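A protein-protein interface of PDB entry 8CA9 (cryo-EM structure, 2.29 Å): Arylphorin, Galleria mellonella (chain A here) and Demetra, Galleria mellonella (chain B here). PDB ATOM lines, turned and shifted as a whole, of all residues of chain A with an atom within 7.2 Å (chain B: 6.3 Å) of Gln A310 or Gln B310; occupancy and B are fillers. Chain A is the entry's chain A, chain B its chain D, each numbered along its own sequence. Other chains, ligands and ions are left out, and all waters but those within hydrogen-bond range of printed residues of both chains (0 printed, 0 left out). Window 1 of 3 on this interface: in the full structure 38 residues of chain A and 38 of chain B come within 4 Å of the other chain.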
ATOM      1  N   VAL A  96     -33.730 -12.559 -12.740  1.00  0.00           N
ATOM      2  CA  VAL A  96     -33.607 -11.241 -12.129  1.00  0.00           C
ATOM      3  C   VAL A  96     -34.811 -10.985 -11.234  1.00  0.00           C
ATOM      4  O   VAL A  96     -35.962 -11.187 -11.640  1.00  0.00           O
ATOM      5  CB  VAL A  96     -33.477 -10.154 -13.206  1.00  0.00           C
ATOM      6  CG1 VAL A  96     -33.400  -8.778 -12.560  1.00  0.00           C
ATOM      7  CG2 VAL A  96     -32.255 -10.402 -14.075  1.00  0.00           C
ATOM      8  N   ASN A 172     -19.342  -1.058 -13.849  1.00  0.00           N
ATOM      9  CA  ASN A 172     -19.666  -1.063 -15.267  1.00  0.00           C
ATOM     10  C   ASN A 172     -19.281  -2.394 -15.905  1.00  0.00           C
ATOM     11  O   ASN A 172     -18.640  -3.249 -15.288  1.00  0.00           O
ATOM     12  CB  ASN A 172     -18.965   0.090 -15.991  1.00  0.00           C
ATOM     13  CG  ASN A 172     -19.544   1.446 -15.630  1.00  0.00           C
ATOM     14  OD1 ASN A 172     -20.754   1.593 -15.455  1.00  0.00           O
ATOM     15  ND2 ASN A 172     -18.677   2.448 -15.518  1.00  0.00           N
ATOM     16  N   SER A 173     -19.688  -2.553 -17.166  1.00  0.00           N
ATOM     17  CA  SER A 173     -19.584  -3.852 -17.822  1.00  0.00           C
ATOM     18  C   SER A 173     -18.140  -4.234 -18.121  1.00  0.00           C
ATOM     19  O   SER A 173     -17.817  -5.424 -18.165  1.00  0.00           O
ATOM     20  CB  SER A 173     -20.410  -3.846 -19.109  1.00  0.00           C
ATOM     21  OG  SER A 173     -19.979  -2.822 -19.988  1.00  0.00           O
ATOM     22  N   ASP A 174     -17.260  -3.255 -18.339  1.00  0.00           N
ATOM     23  CA  ASP A 174     -15.883  -3.569 -18.715  1.00  0.00           C
ATOM     24  C   ASP A 174     -15.138  -4.263 -17.577  1.00  0.00           C
ATOM     25  O   ASP A 174     -14.455  -5.274 -17.787  1.00  0.00           O
ATOM     26  CB  ASP A 174     -15.157  -2.290 -19.137  1.00  0.00           C
ATOM     27  CG  ASP A 174     -15.254  -1.191 -18.096  1.00  0.00           C
ATOM     28  OD1 ASP A 174     -15.935  -1.397 -17.071  1.00  0.00           O
ATOM     29  OD2 ASP A 174     -14.648  -0.118 -18.305  1.00  0.00           O
ATOM     30  N   LEU A 176     -16.455  -5.859 -15.052  1.00  0.00           N
ATOM     31  CA  LEU A 176     -17.069  -7.168 -14.862  1.00  0.00           C
ATOM     32  C   LEU A 176     -16.581  -8.155 -15.912  1.00  0.00           C
ATOM     33  O   LEU A 176     -16.356  -9.332 -15.611  1.00  0.00           O
ATOM     34  CB  LEU A 176     -18.592  -7.041 -14.906  1.00  0.00           C
ATOM     35  CG  LEU A 176     -19.383  -8.291 -14.514  1.00  0.00           C
ATOM     36  CD1 LEU A 176     -19.085  -8.688 -13.075  1.00  0.00           C
ATOM     37  CD2 LEU A 176     -20.875  -8.069 -14.712  1.00  0.00           C
ATOM     38  N   SER A 177     -16.421  -7.696 -17.155  1.00  0.00           N
ATOM     39  CA  SER A 177     -15.893  -8.556 -18.209  1.00  0.00           C
ATOM     40  C   SER A 177     -14.481  -9.015 -17.874  1.00  0.00           C
ATOM     41  O   SER A 177     -14.140 -10.192 -18.039  1.00  0.00           O
ATOM     42  CB  SER A 177     -15.909  -7.812 -19.545  1.00  0.00           C
ATOM     43  OG  SER A 177     -15.515  -8.663 -20.607  1.00  0.00           O
ATOM     44  N   LYS A 178     -13.643  -8.090 -17.406  1.00  0.00           N
ATOM     45  CA  LYS A 178     -12.283  -8.460 -17.024  1.00  0.00           C
ATOM     46  C   LYS A 178     -12.292  -9.481 -15.891  1.00  0.00           C
ATOM     47  O   LYS A 178     -11.541 -10.465 -15.919  1.00  0.00           O
ATOM     48  CB  LYS A 178     -11.494  -7.215 -16.616  1.00  0.00           C
ATOM     49  CG  LYS A 178     -11.189  -6.269 -17.766  1.00  0.00           C
ATOM     50  CD  LYS A 178     -10.463  -5.021 -17.287  1.00  0.00           C
ATOM     51  CE  LYS A 178     -10.121  -4.100 -18.447  1.00  0.00           C
ATOM     52  NZ  LYS A 178      -9.461  -2.842 -18.002  1.00  0.00           N
ATOM     53  N   TYR A 180     -14.689 -11.612 -15.079  1.00  0.00           N
ATOM     54  CA  TYR A 180     -15.172 -12.893 -15.586  1.00  0.00           C
ATOM     55  C   TYR A 180     -14.099 -13.603 -16.399  1.00  0.00           C
ATOM     56  O   TYR A 180     -13.948 -14.826 -16.302  1.00  0.00           O
ATOM     57  CB  TYR A 180     -16.432 -12.688 -16.431  1.00  0.00           C
ATOM     58  CG  TYR A 180     -17.685 -12.347 -15.647  1.00  0.00           C
ATOM     59  CD1 TYR A 180     -17.708 -12.403 -14.258  1.00  0.00           C
ATOM     60  CD2 TYR A 180     -18.852 -11.980 -16.303  1.00  0.00           C
ATOM     61  CE1 TYR A 180     -18.852 -12.096 -13.549  1.00  0.00           C
ATOM     62  CE2 TYR A 180     -20.000 -11.671 -15.600  1.00  0.00           C
ATOM     63  CZ  TYR A 180     -19.995 -11.732 -14.226  1.00  0.00           C
ATOM     64  OH  TYR A 180     -21.138 -11.424 -13.525  1.00  0.00           O
ATOM     65  N   ARG A 181     -13.349 -12.858 -17.214  1.00  0.00           N
ATOM     66  CA  ARG A 181     -12.274 -13.475 -17.983  1.00  0.00           C
ATOM     67  C   ARG A 181     -11.214 -14.062 -17.059  1.00  0.00           C
ATOM     68  O   ARG A 181     -10.733 -15.180 -17.276  1.00  0.00           O
ATOM     69  CB  ARG A 181     -11.649 -12.453 -18.935  1.00  0.00           C
ATOM     70  CG  ARG A 181     -10.437 -12.986 -19.685  1.00  0.00           C
ATOM     71  CD  ARG A 181      -9.981 -12.046 -20.787  1.00  0.00           C
ATOM     72  NE  ARG A 181      -8.785 -12.545 -21.454  1.00  0.00           N
ATOM     73  CZ  ARG A 181      -8.207 -11.964 -22.496  1.00  0.00           C
ATOM     74  NH1 ARG A 181      -8.696 -10.857 -23.031  1.00  0.00           N
ATOM     75  NH2 ARG A 181      -7.110 -12.508 -23.016  1.00  0.00           N
ATOM     76  N   MET A 184     -12.592 -17.247 -15.511  1.00  0.00           N
ATOM     77  CA  MET A 184     -12.619 -18.346 -16.470  1.00  0.00           C
ATOM     78  C   MET A 184     -11.224 -18.887 -16.746  1.00  0.00           C
ATOM     79  O   MET A 184     -11.048 -20.102 -16.881  1.00  0.00           O
ATOM     80  CB  MET A 184     -13.277 -17.890 -17.774  1.00  0.00           C
ATOM     81  CG  MET A 184     -14.793 -17.805 -17.701  1.00  0.00           C
ATOM     82  SD  MET A 184     -15.576 -17.478 -19.293  1.00  0.00           S
ATOM     83  CE  MET A 184     -15.377 -15.704 -19.427  1.00  0.00           C
ATOM     84  N   LEU A 305     -24.366   0.981 -19.046  1.00  0.00           N
ATOM     85  CA  LEU A 305     -23.538  -0.193 -19.321  1.00  0.00           C
ATOM     86  C   LEU A 305     -23.615  -1.189 -18.170  1.00  0.00           C
ATOM     87  O   LEU A 305     -22.600  -1.625 -17.627  1.00  0.00           O
ATOM     88  CB  LEU A 305     -22.097   0.229 -19.585  1.00  0.00           C
ATOM     89  CG  LEU A 305     -21.872   1.130 -20.804  1.00  0.00           C
ATOM     90  CD1 LEU A 305     -20.400   1.483 -20.939  1.00  0.00           C
ATOM     91  CD2 LEU A 305     -22.380   0.469 -22.075  1.00  0.00           C
ATOM     92  N   LEU A 306     -24.835  -1.558 -17.790  1.00  0.00           N
ATOM     93  CA  LEU A 306     -25.089  -2.459 -16.679  1.00  0.00           C
ATOM     94  C   LEU A 306     -25.805  -3.704 -17.184  1.00  0.00           C
ATOM     95  O   LEU A 306     -26.579  -3.648 -18.145  1.00  0.00           O
ATOM     96  CB  LEU A 306     -25.935  -1.778 -15.596  1.00  0.00           C
ATOM     97  CG  LEU A 306     -25.324  -0.542 -14.930  1.00  0.00           C
ATOM     98  CD1 LEU A 306     -26.397   0.263 -14.216  1.00  0.00           C
ATOM     99  CD2 LEU A 306     -24.225  -0.943 -13.960  1.00  0.00           C
ATOM    100  N   SER A 307     -25.542  -4.831 -16.527  1.00  0.00           N
ATOM    101  CA  SER A 307     -26.153  -6.093 -16.916  1.00  0.00           C
ATOM    102  C   SER A 307     -26.293  -6.987 -15.694  1.00  0.00           C
ATOM    103  O   SER A 307     -25.422  -7.014 -14.821  1.00  0.00           O
ATOM    104  CB  SER A 307     -25.328  -6.803 -17.998  1.00  0.00           C
ATOM    105  OG  SER A 307     -24.061  -7.198 -17.500  1.00  0.00           O
ATOM    106  N   SER A 308     -27.404  -7.717 -15.644  1.00  0.00           N
ATOM    107  CA  SER A 308     -27.663  -8.705 -14.606  1.00  0.00           C
ATOM    108  C   SER A 308     -27.979 -10.032 -15.277  1.00  0.00           C
ATOM    109  O   SER A 308     -28.898 -10.111 -16.098  1.00  0.00           O
ATOM    110  CB  SER A 308     -28.820  -8.273 -13.699  1.00  0.00           C
ATOM    111  OG  SER A 308     -29.986  -8.003 -14.455  1.00  0.00           O
ATOM    112  N   TYR A 309     -27.222 -11.070 -14.923  1.00  0.00           N
ATOM    113  CA  TYR A 309     -27.330 -12.372 -15.582  1.00  0.00           C
ATOM    114  C   TYR A 309     -27.143 -12.229 -17.091  1.00  0.00           C
ATOM    115  O   TYR A 309     -27.817 -12.888 -17.886  1.00  0.00           O
ATOM    116  CB  TYR A 309     -28.666 -13.046 -15.262  1.00  0.00           C
ATOM    117  CG  TYR A 309     -28.867 -13.347 -13.794  1.00  0.00           C
ATOM    118  CD1 TYR A 309     -28.354 -14.505 -13.226  1.00  0.00           C
ATOM    119  CD2 TYR A 309     -29.574 -12.475 -12.977  1.00  0.00           C
ATOM    120  CE1 TYR A 309     -28.536 -14.784 -11.885  1.00  0.00           C
ATOM    121  CE2 TYR A 309     -29.761 -12.746 -11.636  1.00  0.00           C
ATOM    122  CZ  TYR A 309     -29.240 -13.902 -11.095  1.00  0.00           C
ATOM    123  OH  TYR A 309     -29.424 -14.175  -9.759  1.00  0.00           O
ATOM    124  N   GLN A 310     -26.218 -11.355 -17.489  1.00  0.00           N
ATOM    125  CA  GLN A 310     -25.898 -11.051 -18.880  1.00  0.00           C
ATOM    126  C   GLN A 310     -27.056 -10.405 -19.630  1.00  0.00           C
ATOM    127  O   GLN A 310     -26.975 -10.243 -20.855  1.00  0.00           O
ATOM    128  CB  GLN A 310     -25.439 -12.300 -19.641  1.00  0.00           C
ATOM    129  CG  GLN A 310     -23.931 -12.452 -19.727  1.00  0.00           C
ATOM    130  CD  GLN A 310     -23.257 -12.347 -18.376  1.00  0.00           C
ATOM    131  OE1 GLN A 310     -23.541 -13.123 -17.464  1.00  0.00           O
ATOM    132  NE2 GLN A 310     -22.361 -11.376 -18.238  1.00  0.00           N
ATOM    133  N   LEU A 311     -28.127 -10.024 -18.939  1.00  0.00           N
ATOM    134  CA  LEU A 311     -29.235  -9.332 -19.580  1.00  0.00           C
ATOM    135  C   LEU A 311     -28.990  -7.830 -19.522  1.00  0.00           C
ATOM    136  O   LEU A 311     -28.871  -7.279 -18.421  1.00  0.00           O
ATOM    137  CB  LEU A 311     -30.551  -9.669 -18.900  1.00  0.00           C
ATOM    138  CG  LEU A 311     -31.024 -11.122 -19.001  1.00  0.00           C
ATOM    139  CD1 LEU A 311     -32.363 -11.286 -18.302  1.00  0.00           C
ATOM    140  CD2 LEU A 311     -31.118 -11.568 -20.452  1.00  0.00           C
ATOM    141  N   PRO A 312     -28.899  -7.137 -20.656  1.00  0.00           N
ATOM    142  CA  PRO A 312     -28.590  -5.706 -20.613  1.00  0.00           C
ATOM    143  C   PRO A 312     -29.712  -4.896 -19.985  1.00  0.00           C
ATOM    144  O   PRO A 312     -30.893  -5.241 -20.080  1.00  0.00           O
ATOM    145  CB  PRO A 312     -28.401  -5.342 -22.089  1.00  0.00           C
ATOM    146  CG  PRO A 312     -29.221  -6.334 -22.824  1.00  0.00           C
ATOM    147  CD  PRO A 312     -29.133  -7.605 -22.033  1.00  0.00           C
ATOM    148  N   PHE A 313     -29.323  -3.805 -19.332  1.00  0.00           N
ATOM    149  CA  PHE A 313     -30.294  -2.862 -18.801  1.00  0.00           C
ATOM    150  C   PHE A 313     -30.940  -2.072 -19.935  1.00  0.00           C
ATOM    151  O   PHE A 313     -30.332  -1.835 -20.983  1.00  0.00           O
ATOM    152  CB  PHE A 313     -29.626  -1.908 -17.812  1.00  0.00           C
ATOM    153  CG  PHE A 313     -29.544  -2.445 -16.411  1.00  0.00           C
ATOM    154  CD1 PHE A 313     -29.043  -3.712 -16.167  1.00  0.00           C
ATOM    155  CD2 PHE A 313     -29.959  -1.676 -15.338  1.00  0.00           C
ATOM    156  CE1 PHE A 313     -28.966  -4.204 -14.879  1.00  0.00           C
ATOM    157  CE2 PHE A 313     -29.883  -2.163 -14.048  1.00  0.00           C
ATOM    158  CZ  PHE A 313     -29.386  -3.427 -13.818  1.00  0.00           C
ATOM    159  N   TYR A 487     -19.065 -16.932 -10.264  1.00  0.00           N
ATOM    160  CA  TYR A 487     -19.458 -18.268  -9.839  1.00  0.00           C
ATOM    161  C   TYR A 487     -18.206 -19.102  -9.601  1.00  0.00           C
ATOM    162  O   TYR A 487     -17.315 -19.151 -10.455  1.00  0.00           O
ATOM    163  CB  TYR A 487     -20.352 -18.936 -10.886  1.00  0.00           C
ATOM    164  CG  TYR A 487     -21.709 -18.287 -11.039  1.00  0.00           C
ATOM    165  CD1 TYR A 487     -22.769 -18.646 -10.217  1.00  0.00           C
ATOM    166  CD2 TYR A 487     -21.932 -17.317 -12.007  1.00  0.00           C
ATOM    167  CE1 TYR A 487     -24.011 -18.058 -10.353  1.00  0.00           C
ATOM    168  CE2 TYR A 487     -23.172 -16.723 -12.150  1.00  0.00           C
ATOM    169  CZ  TYR A 487     -24.208 -17.097 -11.321  1.00  0.00           C
ATOM    170  OH  TYR A 487     -25.444 -16.508 -11.460  1.00  0.00           O
ATOM    171  N   SER B 173     -28.078 -13.799 -25.158  1.00  0.00           N
ATOM    172  CA  SER B 173     -27.267 -13.570 -23.967  1.00  0.00           C
ATOM    173  C   SER B 173     -27.459 -14.654 -22.912  1.00  0.00           C
ATOM    174  O   SER B 173     -26.532 -14.933 -22.148  1.00  0.00           O
ATOM    175  CB  SER B 173     -27.590 -12.195 -23.381  1.00  0.00           C
ATOM    176  OG  SER B 173     -27.262 -11.166 -24.299  1.00  0.00           O
ATOM    177  N   ASP B 174     -28.645 -15.261 -22.837  1.00  0.00           N
ATOM    178  CA  ASP B 174     -28.909 -16.248 -21.790  1.00  0.00           C
ATOM    179  C   ASP B 174     -28.054 -17.500 -21.970  1.00  0.00           C
ATOM    180  O   ASP B 174     -27.450 -17.998 -21.010  1.00  0.00           O
ATOM    181  CB  ASP B 174     -30.393 -16.610 -21.778  1.00  0.00           C
ATOM    182  CG  ASP B 174     -30.901 -17.032 -23.143  1.00  0.00           C
ATOM    183  OD1 ASP B 174     -30.105 -17.013 -24.105  1.00  0.00           O
ATOM    184  OD2 ASP B 174     -32.095 -17.381 -23.255  1.00  0.00           O
ATOM    185  N   LEU B 176     -25.260 -17.822 -23.662  1.00  0.00           N
ATOM    186  CA  LEU B 176     -23.871 -17.460 -23.414  1.00  0.00           C
ATOM    187  C   LEU B 176     -23.599 -17.298 -21.925  1.00  0.00           C
ATOM    188  O   LEU B 176     -22.515 -17.649 -21.452  1.00  0.00           O
ATOM    189  CB  LEU B 176     -23.527 -16.173 -24.160  1.00  0.00           C
ATOM    190  CG  LEU B 176     -22.055 -15.762 -24.140  1.00  0.00           C
ATOM    191  CD1 LEU B 176     -21.194 -16.806 -24.833  1.00  0.00           C
ATOM    192  CD2 LEU B 176     -21.878 -14.401 -24.788  1.00  0.00           C
ATOM    193  N   ALA B 177     -24.565 -16.764 -21.176  1.00  0.00           N
ATOM    194  CA  ALA B 177     -24.405 -16.637 -19.732  1.00  0.00           C
ATOM    195  C   ALA B 177     -24.277 -18.006 -19.081  1.00  0.00           C
ATOM    196  O   ALA B 177     -23.430 -18.218 -18.204  1.00  0.00           O
ATOM    197  CB  ALA B 177     -25.591 -15.875 -19.145  1.00  0.00           C
ATOM    198  N   ASN B 180     -20.830 -19.370 -19.908  1.00  0.00           N
ATOM    199  CA  ASN B 180     -19.802 -18.709 -19.112  1.00  0.00           C
ATOM    200  C   ASN B 180     -19.829 -19.192 -17.669  1.00  0.00           C
ATOM    201  O   ASN B 180     -18.776 -19.367 -17.046  1.00  0.00           O
ATOM    202  CB  ASN B 180     -19.983 -17.191 -19.175  1.00  0.00           C
ATOM    203  CG  ASN B 180     -19.671 -16.623 -20.546  1.00  0.00           C
ATOM    204  OD1 ASN B 180     -19.012 -17.266 -21.362  1.00  0.00           O
ATOM    205  ND2 ASN B 180     -20.137 -15.406 -20.802  1.00  0.00           N
ATOM    206  N   LEU B 305     -30.754  -8.862 -27.506  1.00  0.00           N
ATOM    207  CA  LEU B 305     -30.103  -9.470 -26.347  1.00  0.00           C
ATOM    208  C   LEU B 305     -28.753 -10.049 -26.773  1.00  0.00           C
ATOM    209  O   LEU B 305     -28.513 -11.257 -26.743  1.00  0.00           O
ATOM    210  CB  LEU B 305     -31.004 -10.537 -25.731  1.00  0.00           C
ATOM    211  CG  LEU B 305     -32.374 -10.068 -25.236  1.00  0.00           C
ATOM    212  CD1 LEU B 305     -33.155 -11.228 -24.643  1.00  0.00           C
ATOM    213  CD2 LEU B 305     -32.226  -8.948 -24.219  1.00  0.00           C
ATOM    214  N   THR B 307     -24.302  -9.283 -26.832  1.00  0.00           N
ATOM    215  CA  THR B 307     -23.190  -8.622 -26.169  1.00  0.00           C
ATOM    216  C   THR B 307     -21.884  -9.090 -26.792  1.00  0.00           C
ATOM    217  O   THR B 307     -21.752 -10.246 -27.203  1.00  0.00           O
ATOM    218  CB  THR B 307     -23.170  -8.910 -24.660  1.00  0.00           C
ATOM    219  OG1 THR B 307     -23.139 -10.326 -24.439  1.00  0.00           O
ATOM    220  CG2 THR B 307     -24.392  -8.319 -23.974  1.00  0.00           C
ATOM    221  N   THR B 308     -20.920  -8.175 -26.858  1.00  0.00           N
ATOM    222  CA  THR B 308     -19.552  -8.487 -27.252  1.00  0.00           C
ATOM    223  C   THR B 308     -18.623  -7.846 -26.233  1.00  0.00           C
ATOM    224  O   THR B 308     -18.682  -6.632 -26.014  1.00  0.00           O
ATOM    225  CB  THR B 308     -19.243  -7.986 -28.667  1.00  0.00           C
ATOM    226  OG1 THR B 308     -17.881  -8.286 -28.997  1.00  0.00           O
ATOM    227  CG2 THR B 308     -19.472  -6.485 -28.782  1.00  0.00           C
ATOM    228  N   HIS B 309     -17.777  -8.661 -25.604  1.00  0.00           N
ATOM    229  CA  HIS B 309     -16.940  -8.208 -24.494  1.00  0.00           C
ATOM    230  C   HIS B 309     -17.788  -7.622 -23.370  1.00  0.00           C
ATOM    231  O   HIS B 309     -17.365  -6.699 -22.671  1.00  0.00           O
ATOM    232  CB  HIS B 309     -15.900  -7.187 -24.962  1.00  0.00           C
ATOM    233  CG  HIS B 309     -14.990  -7.699 -26.035  1.00  0.00           C
ATOM    234  ND1 HIS B 309     -13.853  -8.427 -25.761  1.00  0.00           N
ATOM    235  CD2 HIS B 309     -15.048  -7.585 -27.383  1.00  0.00           C
ATOM    236  CE1 HIS B 309     -13.249  -8.741 -26.893  1.00  0.00           C
ATOM    237  NE2 HIS B 309     -13.954  -8.242 -27.892  1.00  0.00           N
ATOM    238  N   GLN B 310     -18.998  -8.155 -23.196  1.00  0.00           N
ATOM    239  CA  GLN B 310     -19.988  -7.729 -22.212  1.00  0.00           C
ATOM    240  C   GLN B 310     -20.577  -6.360 -22.522  1.00  0.00           C
ATOM    241  O   GLN B 310     -21.407  -5.873 -21.745  1.00  0.00           O
ATOM    242  CB  GLN B 310     -19.420  -7.708 -20.785  1.00  0.00           C
ATOM    243  CG  GLN B 310     -18.915  -9.059 -20.303  1.00  0.00           C
ATOM    244  CD  GLN B 310     -20.020 -10.090 -20.193  1.00  0.00           C
ATOM    245  OE1 GLN B 310     -21.202  -9.750 -20.170  1.00  0.00           O
ATOM    246  NE2 GLN B 310     -19.639 -11.360 -20.128  1.00  0.00           N
ATOM    247  N   ILE B 311     -20.185  -5.721 -23.621  1.00  0.00           N
ATOM    248  CA  ILE B 311     -20.733  -4.420 -23.992  1.00  0.00           C
ATOM    249  C   ILE B 311     -22.076  -4.645 -24.678  1.00  0.00           C
ATOM    250  O   ILE B 311     -22.139  -5.361 -25.688  1.00  0.00           O
ATOM    251  CB  ILE B 311     -19.768  -3.641 -24.900  1.00  0.00           C
ATOM    252  CG1 ILE B 311     -18.380  -3.546 -24.257  1.00  0.00           C
ATOM    253  CG2 ILE B 311     -20.314  -2.251 -25.183  1.00  0.00           C
ATOM    254  CD1 ILE B 311     -18.363  -2.876 -22.896  1.00  0.00           C
ATOM    255  N   PRO B 312     -23.168  -4.069 -24.179  1.00  0.00           N
ATOM    256  CA  PRO B 312     -24.477  -4.333 -24.785  1.00  0.00           C
ATOM    257  C   PRO B 312     -24.607  -3.717 -26.169  1.00  0.00           C
ATOM    258  O   PRO B 312     -24.003  -2.687 -26.481  1.00  0.00           O
ATOM    259  CB  PRO B 312     -25.457  -3.692 -23.798  1.00  0.00           C
ATOM    260  CG  PRO B 312     -24.677  -2.611 -23.152  1.00  0.00           C
ATOM    261  CD  PRO B 312     -23.268  -3.123 -23.053  1.00  0.00           C
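Gln A310 touches three residues of chain B.
Gln B310 touches just these residues of chain A: Ser A173 (3.5 Å), Ser A177 (3.3 Å), Tyr A180 (3.95 Å) and Gln A310 (2.8 Å).
Printed residues of chain A within 4 Å of Ser B173: Gln A310.
Of the printed residues of chain B, Ser A177 touches His B309 and Gln B310.
Of the printed residues of chain B, Tyr A309 touches Ala B177.
Printed residues of chain A within 4 Å of Pro B312: Leu A305 (3.8 Å) and Pro A312 (3.8 Å).
Printed residues of chain B within 4 Å of Leu A305: Pro B312.
The nearest residue of chain B that does not touch Gln A310 is Thr B307 (4.5 Å).
The nearest residue of chain A that does not touch Gln B310 is Ser A307 (4.7 Å).
The nearest printed residue of chain B that does not touch Ser A173 is Pro B312 (4.5 Å).
The side-chain hydroxyl (OG) of Ser A177 sits at hydrogen-bond distance from the backbone carbonyl oxygen (O) of His B309 (3.4 Å).
NE2 of Gln A310 lies within hydrogen-bond range of OE1 of Gln B310, 2.8 Å away.
The backbone carbonyl oxygen of Leu A305 is in hydrogen-bond range of the backbone NH of Ser A173 (3.1 Å).
The backbone carbonyl oxygen (O) of Leu B305 lies within hydrogen-bond range of the side-chain hydroxyl (OG) of Ser B173 (2.7 Å).
CB of Ser A173 touches O of Gln B310, at 3.5 Å.
OG of Ser A173 touches CD1 of Ile B311, 3.3 Å away.
Ser A177 touches Gln B310.
CD2 of Tyr A180 touches NE2 of Gln B310 (3.95 Å).
Pro B312 touches Leu A305.
Tyr A309 touches Ala B177 (O to CB, 3.9 Å).
CB of Ser B173 touches O of Gln A310, 3.3 Å away.
Ala B177 touches Gln A310.
Pro A312 touches Pro B312.
Along chain B the printed residues that touch a printed residue of chain A span positions 173 to 312.
Printed residues of chain A that touch a printed residue of chain B: Ser A173, Ser A177, Tyr A180, Leu A305, Tyr A309, Gln A310 and Pro A312.
Hydrophobic or aromatic side chains of chain A within 4 Å of the printed part of chain B: Tyr A180, Leu A305 and Pro A312.
Among the printed residues, no Asp or Glu carboxylate lies within 4 Å of a Lys or Arg side-chain nitrogen of the other chain.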
